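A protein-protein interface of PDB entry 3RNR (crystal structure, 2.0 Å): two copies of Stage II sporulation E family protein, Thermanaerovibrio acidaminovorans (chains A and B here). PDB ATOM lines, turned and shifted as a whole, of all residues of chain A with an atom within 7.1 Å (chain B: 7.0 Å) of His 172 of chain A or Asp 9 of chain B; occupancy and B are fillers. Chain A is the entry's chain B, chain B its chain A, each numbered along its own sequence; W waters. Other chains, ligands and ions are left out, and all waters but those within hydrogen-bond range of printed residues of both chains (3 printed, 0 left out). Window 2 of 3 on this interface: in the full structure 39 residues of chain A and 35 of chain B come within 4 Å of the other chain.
The guanidinium group of Arg 82 of chain B is in salt-bridge range of the side-chain carboxylate of Asp 9 of chain B, 3.8 Å away. NE2 of His 172 of chain A sits at hydrogen-bond distance from OD2 of Asp 26 of chain A (2.9 Å). OG1 of Thr 205 of chain A is in hydrogen-bond range of OD1 of Asp 174 of chain A, 2.8 Å away. NE2 of His 172 of chain A lies close to OG of Ser 170 of chain A, 3.4 Å away. The backbone carbonyl oxygen (O) of Asp 9 of chain B is in hydrogen-bond range of the backbone NH (N) of Leu 81 of chain B.
The side-chain carboxylate of Asp 41 of chain B is in hydrogen-bond range of the side-chain hydroxyl of Ser 1 of chain A. The side-chain carboxylate (OD2) of Asp 9 of chain B is in hydrogen-bond range of a ring nitrogen (ND1) of His 172 of chain A, at 3.1 Å. N of Glu 173 of chain A is in hydrogen-bond range of OD1 of Asp 9 of chain B (2.7 Å).
Water W3 lies within hydrogen-bond range of OG of Ser 1 of chain A (2.6 Å) and OD2 of Asp 41 of chain B (2.7 Å). Water W2 lies within hydrogen-bond range of the backbone carbonyl oxygen (O) of Glu 173 of chain A (2.7 Å), the backbone NH (N) of Asp 9 of chain B (2.9 Å) and the backbone NH (N) of Gly 8 of chain B (3.3 Å). Water W1 lies within hydrogen-bond range of the side-chain hydroxyl (OG1) of Thr 6 of chain B, the side-chain carboxylate (OD1) of Asp 174 of chain A and the backbone NH (N) of Ser 1 of chain A.
Of chain B, only Asp 9 comes within 4 Å of His 172 of chain A. Of the printed residues of chain B, Glu 173 of chain A touches Asp 9 and Leu 81. Printed residues of chain A within 4 Å of Thr 6 of chain B: Ser 1 and Asp 174. Asp 9 of chain B touches just these residues of chain A: His 172 (3.1 Å) and Glu 173 (2.7 Å). Of the printed residues of chain A, Asp 41 of chain B touches Ser 1 (2.6 Å). Printed residues of chain A within 4 Å of Leu 81 of chain B: Glu 173 (3.5 Å) and Asp 174 (3.7 Å). The nearest printed residue of chain B that does not touch Asp 174 of chain A is Asp 9 of chain B (5.7 Å).
No position is printed for both chains.
Hydrophobic or aromatic side chains of chain B within 4 Å of the printed part of chain A: Leu 81. Among the printed residues, no Asp or Glu carboxylate lies within 4 Å of a Lys or Arg side-chain nitrogen of the other chain.
O of Thr 6 of chain B touches CA of Ser 1 of chain A, at 3.2 Å. Ser 1 of chain A touches Gly 7 of chain B. Leu 81 of chain B touches Glu 173 of chain A (CD1 to O, 3.5 Å). CB of Asp 174 of chain A touches OG1 of Thr 6 of chain B, 3.3 Å away. Asp 174 of chain A touches Leu 81 of chain B.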
ATOM      1  N   SER A   1      25.926  26.215 -21.685  1.00  0.00           N
ATOM      2  CA  SER A   1      25.874  27.672 -21.543  1.00  0.00           C
ATOM      3  C   SER A   1      24.618  28.220 -22.185  1.00  0.00           C
ATOM      4  O   SER A   1      24.135  27.668 -23.171  1.00  0.00           O
ATOM      5  CB  SER A   1      27.063  28.326 -22.251  1.00  0.00           C
ATOM      6  OG  SER A   1      28.242  28.166 -21.512  1.00  0.00           O
ATOM      7  N   ASP A  17      26.433  23.895 -26.143  1.00  0.00           N
ATOM      8  CA  ASP A  17      26.999  22.829 -25.308  1.00  0.00           C
ATOM      9  C   ASP A  17      28.185  22.111 -25.923  1.00  0.00           C
ATOM     10  O   ASP A  17      28.164  21.754 -27.099  1.00  0.00           O
ATOM     11  CB  ASP A  17      25.926  21.832 -24.880  1.00  0.00           C
ATOM     12  CG  ASP A  17      25.448  22.086 -23.460  1.00  0.00           C
ATOM     13  OD1 ASP A  17      24.255  22.403 -23.274  1.00  0.00           O
ATOM     14  OD2 ASP A  17      26.285  21.982 -22.549  1.00  0.00           O
ATOM     15  N   ASP A  26      34.075  21.870 -22.961  1.00  0.00           N
ATOM     16  CA  ASP A  26      33.736  23.132 -22.310  1.00  0.00           C
ATOM     17  C   ASP A  26      34.509  24.314 -22.894  1.00  0.00           C
ATOM     18  O   ASP A  26      33.967  25.400 -23.035  1.00  0.00           O
ATOM     19  CB  ASP A  26      33.973  23.035 -20.798  1.00  0.00           C
ATOM     20  CG  ASP A  26      32.797  22.392 -20.059  1.00  0.00           C
ATOM     21  OD1 ASP A  26      31.850  21.909 -20.729  1.00  0.00           O
ATOM     22  OD2 ASP A  26      32.821  22.371 -18.808  1.00  0.00           O
ATOM     23  N   ARG A 169      26.199  16.091 -22.458  1.00  0.00           N
ATOM     24  CA  ARG A 169      26.539  17.356 -21.804  1.00  0.00           C
ATOM     25  C   ARG A 169      27.358  17.226 -20.519  1.00  0.00           C
ATOM     26  O   ARG A 169      27.147  16.311 -19.718  1.00  0.00           O
ATOM     27  CB  ARG A 169      25.268  18.175 -21.551  1.00  0.00           C
ATOM     28  CG  ARG A 169      24.602  18.640 -22.835  1.00  0.00           C
ATOM     29  CD  ARG A 169      23.101  18.836 -22.660  1.00  0.00           C
ATOM     30  NE  ARG A 169      22.763  19.958 -21.796  1.00  0.00           N
ATOM     31  CZ  ARG A 169      21.883  19.889 -20.804  1.00  0.00           C
ATOM     32  NH1 ARG A 169      21.634  20.960 -20.062  1.00  0.00           N
ATOM     33  NH2 ARG A 169      21.255  18.747 -20.554  1.00  0.00           N
ATOM     34  N   SER A 170      28.306  18.146 -20.341  1.00  0.00           N
ATOM     35  CA  SER A 170      29.044  18.269 -19.083  1.00  0.00           C
ATOM     36  C   SER A 170      28.074  18.730 -17.990  1.00  0.00           C
ATOM     37  O   SER A 170      27.136  19.478 -18.261  1.00  0.00           O
ATOM     38  CB  SER A 170      30.199  19.275 -19.226  1.00  0.00           C
ATOM     39  OG  SER A 170      29.728  20.573 -19.607  1.00  0.00           O
ATOM     40  N   LEU A 171      28.305  18.295 -16.754  1.00  0.00           N
ATOM     41  CA  LEU A 171      27.401  18.620 -15.653  1.00  0.00           C
ATOM     42  C   LEU A 171      27.677  20.005 -15.062  1.00  0.00           C
ATOM     43  O   LEU A 171      28.786  20.291 -14.609  1.00  0.00           O
ATOM     44  CB  LEU A 171      27.473  17.543 -14.563  1.00  0.00           C
ATOM     45  CG  LEU A 171      27.265  16.109 -15.064  1.00  0.00           C
ATOM     46  CD1 LEU A 171      27.198  15.129 -13.900  1.00  0.00           C
ATOM     47  CD2 LEU A 171      26.016  16.009 -15.929  1.00  0.00           C
ATOM     48  N   HIS A 172      26.661  20.860 -15.072  1.00  0.00           N
ATOM     49  CA  HIS A 172      26.775  22.198 -14.504  1.00  0.00           C
ATOM     50  C   HIS A 172      25.450  22.642 -13.894  1.00  0.00           C
ATOM     51  O   HIS A 172      24.383  22.162 -14.290  1.00  0.00           O
ATOM     52  CB  HIS A 172      27.198  23.207 -15.580  1.00  0.00           C
ATOM     53  CG  HIS A 172      28.623  23.065 -16.019  1.00  0.00           C
ATOM     54  ND1 HIS A 172      29.680  23.533 -15.275  1.00  0.00           N
ATOM     55  CD2 HIS A 172      29.160  22.513 -17.137  1.00  0.00           C
ATOM     56  CE1 HIS A 172      30.814  23.271 -15.908  1.00  0.00           C
ATOM     57  NE2 HIS A 172      30.523  22.656 -17.039  1.00  0.00           N
ATOM     58  N   GLU A 173      25.532  23.557 -12.929  1.00  0.00           N
ATOM     59  CA  GLU A 173      24.362  24.267 -12.423  1.00  0.00           C
ATOM     60  C   GLU A 173      24.078  25.418 -13.372  1.00  0.00           C
ATOM     61  O   GLU A 173      24.990  26.150 -13.742  1.00  0.00           O
ATOM     62  CB  GLU A 173      24.651  24.838 -11.029  1.00  0.00           C
ATOM     63  CG  GLU A 173      24.517  23.833  -9.901  1.00  0.00           C
ATOM     64  CD  GLU A 173      23.117  23.253  -9.821  1.00  0.00           C
ATOM     65  OE1 GLU A 173      22.150  24.043  -9.706  1.00  0.00           O
ATOM     66  OE2 GLU A 173      22.983  22.012  -9.891  1.00  0.00           O
ATOM     67  N   ASP A 174      22.823  25.590 -13.762  1.00  0.00           N
ATOM     68  CA  ASP A 174      22.463  26.748 -14.576  1.00  0.00           C
ATOM     69  C   ASP A 174      21.065  27.281 -14.246  1.00  0.00           C
ATOM     70  O   ASP A 174      20.467  26.883 -13.255  1.00  0.00           O
ATOM     71  CB  ASP A 174      22.658  26.470 -16.079  1.00  0.00           C
ATOM     72  CG  ASP A 174      21.604  25.535 -16.657  1.00  0.00           C
ATOM     73  OD1 ASP A 174      21.604  25.358 -17.898  1.00  0.00           O
ATOM     74  OD2 ASP A 174      20.783  24.987 -15.884  1.00  0.00           O
ATOM     75  N   ASN A 203      16.390  18.241 -17.480  1.00  0.00           N
ATOM     76  CA  ASN A 203      17.670  18.916 -17.249  1.00  0.00           C
ATOM     77  C   ASN A 203      18.100  19.877 -18.372  1.00  0.00           C
ATOM     78  O   ASN A 203      19.252  20.334 -18.409  1.00  0.00           O
ATOM     79  CB  ASN A 203      18.782  17.930 -16.863  1.00  0.00           C
ATOM     80  CG  ASN A 203      19.102  16.950 -17.970  1.00  0.00           C
ATOM     81  OD1 ASN A 203      18.458  16.946 -19.022  1.00  0.00           O
ATOM     82  ND2 ASN A 203      20.115  16.114 -17.744  1.00  0.00           N
ATOM     83  N   THR A 205      18.926  22.857 -20.969  1.00  0.00           N
ATOM     84  CA  THR A 205      19.324  24.255 -20.867  1.00  0.00           C
ATOM     85  C   THR A 205      18.450  25.044 -21.827  1.00  0.00           C
ATOM     86  O   THR A 205      18.268  24.632 -22.976  1.00  0.00           O
ATOM     87  CB  THR A 205      20.832  24.439 -21.200  1.00  0.00           C
ATOM     88  OG1 THR A 205      21.621  23.779 -20.200  1.00  0.00           O
ATOM     89  CG2 THR A 205      21.213  25.903 -21.207  1.00  0.00           C
ATOM     90  N   THR B   6      24.299  31.995 -18.280  1.00  0.00           N
ATOM     91  CA  THR B   6      24.845  31.088 -17.304  1.00  0.00           C
ATOM     92  C   THR B   6      25.896  30.259 -18.010  1.00  0.00           C
ATOM     93  O   THR B   6      25.731  29.893 -19.178  1.00  0.00           O
ATOM     94  CB  THR B   6      23.753  30.175 -16.711  1.00  0.00           C
ATOM     95  OG1 THR B   6      23.305  29.261 -17.711  1.00  0.00           O
ATOM     96  CG2 THR B   6      22.573  30.990 -16.250  1.00  0.00           C
ATOM     97  N   GLY B   7      27.002  30.023 -17.316  1.00  0.00           N
ATOM     98  CA  GLY B   7      28.035  29.110 -17.776  1.00  0.00           C
ATOM     99  C   GLY B   7      29.013  28.915 -16.628  1.00  0.00           C
ATOM    100  O   GLY B   7      29.132  29.787 -15.766  1.00  0.00           O
ATOM    101  N   GLY B   8      29.725  27.797 -16.616  1.00  0.00           N
ATOM    102  CA  GLY B   8      30.693  27.541 -15.556  1.00  0.00           C
ATOM    103  C   GLY B   8      30.141  27.662 -14.140  1.00  0.00           C
ATOM    104  O   GLY B   8      30.829  28.168 -13.255  1.00  0.00           O
ATOM    105  N   ASP B   9      28.914  27.184 -13.930  1.00  0.00           N
ATOM    106  CA  ASP B   9      28.238  27.228 -12.626  1.00  0.00           C
ATOM    107  C   ASP B   9      27.965  28.642 -12.070  1.00  0.00           C
ATOM    108  O   ASP B   9      27.775  28.838 -10.864  1.00  0.00           O
ATOM    109  CB  ASP B   9      28.994  26.366 -11.612  1.00  0.00           C
ATOM    110  CG  ASP B   9      29.126  24.914 -12.081  1.00  0.00           C
ATOM    111  OD1 ASP B   9      28.085  24.234 -12.211  1.00  0.00           O
ATOM    112  OD2 ASP B   9      30.258  24.462 -12.349  1.00  0.00           O
ATOM    113  N   LYS B  10      27.907  29.622 -12.958  1.00  0.00           N
ATOM    114  CA  LYS B  10      27.551  30.974 -12.545  1.00  0.00           C
ATOM    115  C   LYS B  10      26.468  31.523 -13.441  1.00  0.00           C
ATOM    116  O   LYS B  10      26.368  31.129 -14.608  1.00  0.00           O
ATOM    117  CB  LYS B  10      28.770  31.893 -12.569  1.00  0.00           C
ATOM    118  CG  LYS B  10      29.813  31.525 -11.513  1.00  0.00           C
ATOM    119  CD  LYS B  10      30.317  32.749 -10.773  1.00  0.00           C
ATOM    120  CE  LYS B  10      31.119  33.654 -11.682  1.00  0.00           C
ATOM    121  NZ  LYS B  10      32.231  32.935 -12.368  1.00  0.00           N
ATOM    122  N   ALA B  11      25.642  32.407 -12.884  1.00  0.00           N
ATOM    123  CA  ALA B  11      24.706  33.182 -13.688  1.00  0.00           C
ATOM    124  C   ALA B  11      25.169  34.628 -13.582  1.00  0.00           C
ATOM    125  O   ALA B  11      25.512  35.092 -12.492  1.00  0.00           O
ATOM    126  CB  ALA B  11      23.270  33.026 -13.158  1.00  0.00           C
ATOM    127  N   ASP B  41      31.338  33.769 -18.898  1.00  0.00           N
ATOM    128  CA  ASP B  41      30.976  32.433 -19.327  1.00  0.00           C
ATOM    129  C   ASP B  41      32.094  31.418 -19.049  1.00  0.00           C
ATOM    130  O   ASP B  41      31.817  30.250 -18.794  1.00  0.00           O
ATOM    131  CB  ASP B  41      30.616  32.433 -20.812  1.00  0.00           C
ATOM    132  CG  ASP B  41      30.289  31.038 -21.317  1.00  0.00           C
ATOM    133  OD1 ASP B  41      29.200  30.527 -21.001  1.00  0.00           O
ATOM    134  OD2 ASP B  41      31.125  30.456 -22.019  1.00  0.00           O
ATOM    135  N   GLY B  43      33.984  31.465 -16.458  1.00  0.00           N
ATOM    136  CA  GLY B  43      34.146  31.278 -15.022  1.00  0.00           C
ATOM    137  C   GLY B  43      34.798  32.438 -14.293  1.00  0.00           C
ATOM    138  O   GLY B  43      35.080  32.352 -13.105  1.00  0.00           O
ATOM    139  N   VAL B  79      26.436  35.549  -9.872  1.00  0.00           N
ATOM    140  CA  VAL B  79      26.075  34.759  -8.706  1.00  0.00           C
ATOM    141  C   VAL B  79      26.662  33.367  -8.876  1.00  0.00           C
ATOM    142  O   VAL B  79      26.474  32.732  -9.910  1.00  0.00           O
ATOM    143  CB  VAL B  79      24.552  34.678  -8.550  1.00  0.00           C
ATOM    144  CG1 VAL B  79      24.163  33.735  -7.382  1.00  0.00           C
ATOM    145  CG2 VAL B  79      23.986  36.076  -8.336  1.00  0.00           C
ATOM    146  N   ASN B  80      27.397  32.892  -7.881  1.00  0.00           N
ATOM    147  CA  ASN B  80      27.931  31.543  -7.969  1.00  0.00           C
ATOM    148  C   ASN B  80      26.807  30.600  -7.581  1.00  0.00           C
ATOM    149  O   ASN B  80      26.320  30.643  -6.455  1.00  0.00           O
ATOM    150  CB  ASN B  80      29.134  31.368  -7.028  1.00  0.00           C
ATOM    151  CG  ASN B  80      29.711  29.951  -7.065  1.00  0.00           C
ATOM    152  OD1 ASN B  80      28.985  28.968  -6.932  1.00  0.00           O
ATOM    153  ND2 ASN B  80      31.019  29.851  -7.260  1.00  0.00           N
ATOM    154  N   LEU B  81      26.415  29.732  -8.503  1.00  0.00           N
ATOM    155  CA  LEU B  81      25.234  28.908  -8.295  1.00  0.00           C
ATOM    156  C   LEU B  81      25.509  27.715  -7.384  1.00  0.00           C
ATOM    157  O   LEU B  81      24.575  27.069  -6.910  1.00  0.00           O
ATOM    158  CB  LEU B  81      24.680  28.420  -9.636  1.00  0.00           C
ATOM    159  CG  LEU B  81      24.240  29.536 -10.589  1.00  0.00           C
ATOM    160  CD1 LEU B  81      23.821  28.930 -11.943  1.00  0.00           C
ATOM    161  CD2 LEU B  81      23.120  30.367  -9.971  1.00  0.00           C
ATOM    162  N   ARG B  82      26.782  27.383  -7.192  1.00  0.00           N
ATOM    163  CA  ARG B  82      27.132  26.328  -6.238  1.00  0.00           C
ATOM    164  C   ARG B  82      27.022  26.785  -4.789  1.00  0.00           C
ATOM    165  O   ARG B  82      26.411  26.111  -3.965  1.00  0.00           O
ATOM    166  CB  ARG B  82      28.542  25.792  -6.492  1.00  0.00           C
ATOM    167  CG  ARG B  82      28.682  24.902  -7.723  1.00  0.00           C
ATOM    168  CD  ARG B  82      29.736  23.827  -7.466  1.00  0.00           C
ATOM    169  NE  ARG B  82      30.035  23.020  -8.645  1.00  0.00           N
ATOM    170  CZ  ARG B  82      29.217  22.104  -9.159  1.00  0.00           C
ATOM    171  NH1 ARG B  82      28.029  21.883  -8.610  1.00  0.00           N
ATOM    172  NH2 ARG B  82      29.585  21.415 -10.233  1.00  0.00           N
ATOM    173  N   ASP B  83      27.682  27.891  -4.460  1.00  0.00           N
ATOM    174  CA  ASP B  83      27.639  28.393  -3.087  1.00  0.00           C
ATOM    175  C   ASP B  83      26.697  29.570  -2.782  1.00  0.00           C
ATOM    176  O   ASP B  83      26.611  30.010  -1.644  1.00  0.00           O
ATOM    177  CB  ASP B  83      29.048  28.610  -2.526  1.00  0.00           C
ATOM    178  CG  ASP B  83      29.748  29.796  -3.134  1.00  0.00           C
ATOM    179  OD1 ASP B  83      29.064  30.685  -3.688  1.00  0.00           O
ATOM    180  OD2 ASP B  83      30.994  29.843  -3.044  1.00  0.00           O
HETATM  181  O   HOH W   1      23.894  26.921 -19.067  1.00  0.00           O
HETATM  182  O   HOH W   2      26.692  26.899 -15.707  1.00  0.00           O
HETATM  183  O   HOH W   3      30.623  27.894 -22.589  1.00  0.00           O
